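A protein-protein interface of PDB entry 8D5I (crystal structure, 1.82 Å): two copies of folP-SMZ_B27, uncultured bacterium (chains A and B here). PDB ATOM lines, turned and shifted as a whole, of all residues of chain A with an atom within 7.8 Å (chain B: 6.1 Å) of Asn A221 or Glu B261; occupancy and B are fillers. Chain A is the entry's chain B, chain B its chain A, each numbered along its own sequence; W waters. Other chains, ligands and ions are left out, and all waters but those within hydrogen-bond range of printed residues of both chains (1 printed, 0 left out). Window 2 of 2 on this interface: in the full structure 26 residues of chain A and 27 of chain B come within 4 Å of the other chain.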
ATOM      1  N   PHE A 192      -1.126 -35.516  -1.908  1.00  0.00           N
ATOM      2  CA  PHE A 192       0.116 -34.831  -2.266  1.00  0.00           C
ATOM      3  C   PHE A 192       1.326 -35.559  -1.691  1.00  0.00           C
ATOM      4  O   PHE A 192       2.388 -35.606  -2.324  1.00  0.00           O
ATOM      5  CB  PHE A 192       0.092 -33.376  -1.776  1.00  0.00           C
ATOM      6  CG  PHE A 192      -0.905 -32.508  -2.499  1.00  0.00           C
ATOM      7  CD1 PHE A 192      -0.997 -32.537  -3.883  1.00  0.00           C
ATOM      8  CD2 PHE A 192      -1.775 -31.691  -1.785  1.00  0.00           C
ATOM      9  CE1 PHE A 192      -1.933 -31.753  -4.542  1.00  0.00           C
ATOM     10  CE2 PHE A 192      -2.698 -30.893  -2.443  1.00  0.00           C
ATOM     11  CZ  PHE A 192      -2.779 -30.933  -3.824  1.00  0.00           C
ATOM     12  N   PHE A 217      -8.608 -33.693  -4.720  1.00  0.00           N
ATOM     13  CA  PHE A 217      -7.447 -33.118  -4.046  1.00  0.00           C
ATOM     14  C   PHE A 217      -6.807 -31.990  -4.856  1.00  0.00           C
ATOM     15  O   PHE A 217      -6.021 -31.219  -4.293  1.00  0.00           O
ATOM     16  CB  PHE A 217      -6.412 -34.205  -3.711  1.00  0.00           C
ATOM     17  CG  PHE A 217      -5.631 -34.719  -4.894  1.00  0.00           C
ATOM     18  CD1 PHE A 217      -6.179 -35.628  -5.785  1.00  0.00           C
ATOM     19  CD2 PHE A 217      -4.326 -34.267  -5.112  1.00  0.00           C
ATOM     20  CE1 PHE A 217      -5.438 -36.092  -6.867  1.00  0.00           C
ATOM     21  CE2 PHE A 217      -3.583 -34.728  -6.190  1.00  0.00           C
ATOM     22  CZ  PHE A 217      -4.154 -35.643  -7.074  1.00  0.00           C
ATOM     23  N   LEU A 218      -7.170 -31.857  -6.133  1.00  0.00           N
ATOM     24  CA  LEU A 218      -6.705 -30.826  -7.050  1.00  0.00           C
ATOM     25  C   LEU A 218      -7.586 -29.587  -7.023  1.00  0.00           C
ATOM     26  O   LEU A 218      -7.436 -28.709  -7.883  1.00  0.00           O
ATOM     27  CB  LEU A 218      -6.658 -31.386  -8.472  1.00  0.00           C
ATOM     28  CG  LEU A 218      -5.734 -32.590  -8.661  1.00  0.00           C
ATOM     29  CD1 LEU A 218      -5.917 -33.208 -10.057  1.00  0.00           C
ATOM     30  CD2 LEU A 218      -4.259 -32.219  -8.438  1.00  0.00           C
ATOM     31  N   ALA A 219      -8.503 -29.493  -6.061  1.00  0.00           N
ATOM     32  CA  ALA A 219      -9.345 -28.309  -5.980  1.00  0.00           C
ATOM     33  C   ALA A 219      -8.518 -27.067  -5.638  1.00  0.00           C
ATOM     34  O   ALA A 219      -8.841 -25.969  -6.094  1.00  0.00           O
ATOM     35  CB  ALA A 219     -10.475 -28.536  -4.963  1.00  0.00           C
ATOM     36  N   GLY A 220      -7.446 -27.219  -4.855  1.00  0.00           N
ATOM     37  CA  GLY A 220      -6.594 -26.089  -4.528  1.00  0.00           C
ATOM     38  C   GLY A 220      -7.254 -25.071  -3.606  1.00  0.00           C
ATOM     39  O   GLY A 220      -8.364 -25.268  -3.081  1.00  0.00           O
ATOM     40  N   ASN A 221      -6.542 -23.948  -3.422  1.00  0.00           N
ATOM     41  CA  ASN A 221      -7.041 -22.866  -2.572  1.00  0.00           C
ATOM     42  C   ASN A 221      -8.373 -22.321  -3.064  1.00  0.00           C
ATOM     43  O   ASN A 221      -9.187 -21.860  -2.257  1.00  0.00           O
ATOM     44  CB  ASN A 221      -6.041 -21.702  -2.511  1.00  0.00           C
ATOM     45  CG  ASN A 221      -4.701 -22.097  -1.926  1.00  0.00           C
ATOM     46  OD1 ASN A 221      -3.652 -21.662  -2.414  1.00  0.00           O
ATOM     47  ND2 ASN A 221      -4.724 -22.893  -0.861  1.00  0.00           N
ATOM     48  N   GLU A 222      -8.590 -22.310  -4.377  1.00  0.00           N
ATOM     49  CA  GLU A 222      -9.798 -21.719  -4.932  1.00  0.00           C
ATOM     50  C   GLU A 222     -10.981 -22.687  -4.875  1.00  0.00           C
ATOM     51  O   GLU A 222     -12.086 -22.321  -5.292  1.00  0.00           O
ATOM     52  CB  GLU A 222      -9.568 -21.307  -6.387  1.00  0.00           C
ATOM     53  CG  GLU A 222      -8.467 -20.256  -6.582  1.00  0.00           C
ATOM     54  CD  GLU A 222      -8.023 -20.189  -8.043  1.00  0.00           C
ATOM     55  OE1 GLU A 222      -8.685 -19.496  -8.851  1.00  0.00           O
ATOM     56  OE2 GLU A 222      -7.132 -20.986  -8.419  1.00  0.00           O
ATOM     57  N   LEU A 223     -10.753 -23.910  -4.408  1.00  0.00           N
ATOM     58  CA  LEU A 223     -11.774 -24.952  -4.357  1.00  0.00           C
ATOM     59  C   LEU A 223     -12.425 -25.147  -5.731  1.00  0.00           C
ATOM     60  O   LEU A 223     -13.648 -25.076  -5.895  1.00  0.00           O
ATOM     61  CB  LEU A 223     -12.806 -24.638  -3.269  1.00  0.00           C
ATOM     62  CG  LEU A 223     -12.198 -24.729  -1.861  1.00  0.00           C
ATOM     63  CD1 LEU A 223     -13.190 -24.360  -0.761  1.00  0.00           C
ATOM     64  CD2 LEU A 223     -11.650 -26.145  -1.638  1.00  0.00           C
ATOM     65  N   LEU A 224     -11.571 -25.424  -6.719  1.00  0.00           N
ATOM     66  CA  LEU A 224     -12.020 -25.515  -8.102  1.00  0.00           C
ATOM     67  C   LEU A 224     -12.957 -26.697  -8.312  1.00  0.00           C
ATOM     68  O   LEU A 224     -12.738 -27.790  -7.785  1.00  0.00           O
ATOM     69  CB  LEU A 224     -10.830 -25.635  -9.058  1.00  0.00           C
ATOM     70  CG  LEU A 224      -9.711 -24.592  -8.900  1.00  0.00           C
ATOM     71  CD1 LEU A 224      -8.481 -24.974  -9.720  1.00  0.00           C
ATOM     72  CD2 LEU A 224     -10.226 -23.234  -9.335  1.00  0.00           C
ATOM     73  N   GLY A 232      -4.195 -28.464 -12.945  1.00  0.00           N
ATOM     74  CA  GLY A 232      -3.718 -29.261 -11.821  1.00  0.00           C
ATOM     75  C   GLY A 232      -3.528 -30.724 -12.171  1.00  0.00           C
ATOM     76  O   GLY A 232      -2.599 -31.378 -11.687  1.00  0.00           O
ATOM     77  N   ALA A 235      -0.193 -30.989 -14.055  1.00  0.00           N
ATOM     78  CA  ALA A 235       0.954 -30.870 -13.153  1.00  0.00           C
ATOM     79  C   ALA A 235       1.116 -32.131 -12.312  1.00  0.00           C
ATOM     80  O   ALA A 235       2.232 -32.646 -12.162  1.00  0.00           O
ATOM     81  CB  ALA A 235       0.798 -29.651 -12.242  1.00  0.00           C
ATOM     82  N   VAL B   4       4.851 -19.968  -5.367  1.00  0.00           N
ATOM     83  CA  VAL B   4       5.647 -19.337  -6.416  1.00  0.00           C
ATOM     84  C   VAL B   4       5.026 -17.989  -6.759  1.00  0.00           C
ATOM     85  O   VAL B   4       3.806 -17.796  -6.671  1.00  0.00           O
ATOM     86  CB  VAL B   4       5.747 -20.250  -7.655  1.00  0.00           C
ATOM     87  CG1 VAL B   4       4.445 -20.235  -8.461  1.00  0.00           C
ATOM     88  CG2 VAL B   4       6.941 -19.852  -8.549  1.00  0.00           C
ATOM     89  N   VAL B 256      -0.879 -21.737 -15.552  1.00  0.00           N
ATOM     90  CA  VAL B 256       0.420 -22.047 -14.965  1.00  0.00           C
ATOM     91  C   VAL B 256       0.387 -21.832 -13.454  1.00  0.00           C
ATOM     92  O   VAL B 256       0.980 -22.608 -12.693  1.00  0.00           O
ATOM     93  CB  VAL B 256       1.525 -21.219 -15.650  1.00  0.00           C
ATOM     94  CG1 VAL B 256       2.825 -21.227 -14.811  1.00  0.00           C
ATOM     95  CG2 VAL B 256       1.775 -21.736 -17.066  1.00  0.00           C
ATOM     96  N   ARG B 257      -0.327 -20.799 -12.995  1.00  0.00           N
ATOM     97  CA  ARG B 257      -0.507 -20.590 -11.559  1.00  0.00           C
ATOM     98  C   ARG B 257      -1.172 -21.797 -10.906  1.00  0.00           C
ATOM     99  O   ARG B 257      -0.721 -22.278  -9.860  1.00  0.00           O
ATOM    100  CB  ARG B 257      -1.341 -19.340 -11.290  1.00  0.00           C
ATOM    101  CG  ARG B 257      -1.649 -19.146  -9.810  1.00  0.00           C
ATOM    102  CD  ARG B 257      -2.405 -17.856  -9.505  1.00  0.00           C
ATOM    103  NE  ARG B 257      -3.759 -17.795 -10.059  1.00  0.00           N
ATOM    104  CZ  ARG B 257      -4.799 -18.523  -9.650  1.00  0.00           C
ATOM    105  NH1 ARG B 257      -4.678 -19.459  -8.717  1.00  0.00           N
ATOM    106  NH2 ARG B 257      -5.995 -18.307 -10.193  1.00  0.00           N
ATOM    107  N   ARG B 258      -2.258 -22.293 -11.506  1.00  0.00           N
ATOM    108  CA  ARG B 258      -2.951 -23.438 -10.918  1.00  0.00           C
ATOM    109  C   ARG B 258      -2.074 -24.689 -10.923  1.00  0.00           C
ATOM    110  O   ARG B 258      -2.033 -25.423  -9.929  1.00  0.00           O
ATOM    111  CB  ARG B 258      -4.286 -23.685 -11.627  1.00  0.00           C
ATOM    112  CG  ARG B 258      -5.340 -22.639 -11.251  1.00  0.00           C
ATOM    113  CD  ARG B 258      -6.602 -22.642 -12.112  1.00  0.00           C
ATOM    114  NE  ARG B 258      -7.577 -21.701 -11.558  1.00  0.00           N
ATOM    115  CZ  ARG B 258      -8.709 -21.336 -12.145  1.00  0.00           C
ATOM    116  NH1 ARG B 258      -9.068 -21.826 -13.321  1.00  0.00           N
ATOM    117  NH2 ARG B 258      -9.500 -20.454 -11.536  1.00  0.00           N
ATOM    118  N   GLY B 259      -1.367 -24.953 -12.021  1.00  0.00           N
ATOM    119  CA  GLY B 259      -0.459 -26.089 -12.033  1.00  0.00           C
ATOM    120  C   GLY B 259       0.657 -25.959 -11.010  1.00  0.00           C
ATOM    121  O   GLY B 259       0.996 -26.926 -10.318  1.00  0.00           O
ATOM    122  N   CYS B 260       1.248 -24.763 -10.901  1.00  0.00           N
ATOM    123  CA  CYS B 260       2.339 -24.568  -9.950  1.00  0.00           C
ATOM    124  C   CYS B 260       1.859 -24.678  -8.511  1.00  0.00           C
ATOM    125  O   CYS B 260       2.647 -25.029  -7.622  1.00  0.00           O
ATOM    126  CB  CYS B 260       3.027 -23.217 -10.190  1.00  0.00           C
ATOM    127  SG  CYS B 260       3.981 -23.198 -11.733  1.00  0.00           S
ATOM    128  N   GLU B 261       0.582 -24.379  -8.256  1.00  0.00           N
ATOM    129  CA  GLU B 261       0.059 -24.545  -6.908  1.00  0.00           C
ATOM    130  C   GLU B 261       0.095 -26.016  -6.484  1.00  0.00           C
ATOM    131  O   GLU B 261       0.380 -26.336  -5.316  1.00  0.00           O
ATOM    132  CB  GLU B 261      -1.354 -23.961  -6.833  1.00  0.00           C
ATOM    133  CG  GLU B 261      -1.982 -24.066  -5.461  1.00  0.00           C
ATOM    134  CD  GLU B 261      -3.480 -23.794  -5.470  1.00  0.00           C
ATOM    135  OE1 GLU B 261      -4.026 -23.347  -6.509  1.00  0.00           O
ATOM    136  OE2 GLU B 261      -4.113 -24.059  -4.432  1.00  0.00           O
ATOM    137  N   ILE B 262      -0.154 -26.927  -7.430  1.00  0.00           N
ATOM    138  CA  ILE B 262      -0.035 -28.354  -7.147  1.00  0.00           C
ATOM    139  C   ILE B 262       1.402 -28.724  -6.800  1.00  0.00           C
ATOM    140  O   ILE B 262       1.653 -29.463  -5.842  1.00  0.00           O
ATOM    141  CB  ILE B 262      -0.569 -29.171  -8.342  1.00  0.00           C
ATOM    142  CG1 ILE B 262      -2.022 -28.760  -8.660  1.00  0.00           C
ATOM    143  CG2 ILE B 262      -0.395 -30.652  -8.109  1.00  0.00           C
ATOM    144  CD1 ILE B 262      -2.960 -28.898  -7.497  1.00  0.00           C
ATOM    145  N   ALA B 263       2.373 -28.216  -7.566  1.00  0.00           N
ATOM    146  CA  ALA B 263       3.774 -28.496  -7.259  1.00  0.00           C
ATOM    147  C   ALA B 263       4.159 -27.985  -5.871  1.00  0.00           C
ATOM    148  O   ALA B 263       4.875 -28.666  -5.126  1.00  0.00           O
ATOM    149  CB  ALA B 263       4.681 -27.885  -8.329  1.00  0.00           C
ATOM    150  N   THR B 264       3.696 -26.788  -5.505  1.00  0.00           N
ATOM    151  CA  THR B 264       3.976 -26.280  -4.166  1.00  0.00           C
ATOM    152  C   THR B 264       3.392 -27.187  -3.095  1.00  0.00           C
ATOM    153  O   THR B 264       4.046 -27.452  -2.081  1.00  0.00           O
ATOM    154  CB  THR B 264       3.449 -24.849  -4.028  1.00  0.00           C
ATOM    155  OG1 THR B 264       4.028 -24.032  -5.059  1.00  0.00           O
ATOM    156  CG2 THR B 264       3.782 -24.269  -2.662  1.00  0.00           C
ATOM    157  N   ALA B 265       2.167 -27.691  -3.312  1.00  0.00           N
ATOM    158  CA  ALA B 265       1.520 -28.564  -2.333  1.00  0.00           C
ATOM    159  C   ALA B 265       2.272 -29.879  -2.161  1.00  0.00           C
ATOM    160  O   ALA B 265       2.385 -30.396  -1.042  1.00  0.00           O
ATOM    161  CB  ALA B 265       0.073 -28.838  -2.749  1.00  0.00           C
ATOM    162  N   ILE B 266       2.765 -30.447  -3.265  1.00  0.00           N
ATOM    163  CA  ILE B 266       3.552 -31.674  -3.200  1.00  0.00           C
ATOM    164  C   ILE B 266       4.861 -31.441  -2.451  1.00  0.00           C
ATOM    165  O   ILE B 266       5.358 -32.337  -1.754  1.00  0.00           O
ATOM    166  CB  ILE B 266       3.772 -32.222  -4.627  1.00  0.00           C
ATOM    167  CG1 ILE B 266       2.416 -32.648  -5.212  1.00  0.00           C
ATOM    168  CG2 ILE B 266       4.775 -33.384  -4.628  1.00  0.00           C
ATOM    169  CD1 ILE B 266       2.416 -32.959  -6.708  1.00  0.00           C
HETATM  170  O   HOH W   1      -6.465 -22.977  -6.477  1.00  0.00           O
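N of Leu A224 sits at hydrogen-bond distance from O of Ala A219 (2.9 Å).
No position is printed for both chains. Of the 10 pairs that touch across the chains among the printed residues, none has its exchanged pair printed and touching as well.
Water W1 lies within hydrogen-bond range of the side-chain carboxylate (OE1) of Glu B261 (2.5 Å), the side-chain carboxylate (OE2) of Glu A222 (2.9 Å) and the backbone NH (N) of Asn A221 (3.2 Å).
Among the printed residues, pairs that only touch across the chains: Gly A220 with Glu B261 (3.2 Å), Ala A235 with Gly B259 (3.3 Å), Phe A192 with Ala B265 (3.5 Å), Leu A224 with Arg B258 (3.6 Å), Gly A232 with Ile B262 (3.6 Å), Phe A192 with Ile B266 (3.7 Å) and Leu A218 with Ile B262 (3.7 Å).
The guanidinium group (NH1) of Arg B257 is in salt-bridge range of the side-chain carboxylate (OE2) of Glu A222 (2.9 Å). The side-chain carboxylate (OE2) of Glu B261 lies within hydrogen-bond range of the backbone NH (N) of Asn A221 (2.6 Å). NH2 of Arg B258 is in salt-bridge range of OE1 of Glu A222, 3.0 Å away.
Hydrophobic or aromatic side chains of chain A within 4 Å of the printed part of chain B: Phe A192, Leu A218, Leu A224 and Ala A235. Of the 12 printed residues of chain B, 7 touch a printed residue of chain A. Hydrophobic or aromatic side chains of chain B that line the printed part of chain A: Ile B262, Ala B265 and Ile B266.
Asn A221 touches just one residue of chain B: Glu B261. Glu B261 touches just these residues of chain A: Gly A220 and Asn A221. Of the printed residues of chain B, Leu A224 touches Arg B258 (3.6 Å). Of the printed residues of chain B, Ala A235 touches Gly B259 (3.3 Å). Phe A217 touches none of the printed residues of chain B. The nearest printed residue of chain B that does not touch Asn A221 is Arg B257 (6.7 Å).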
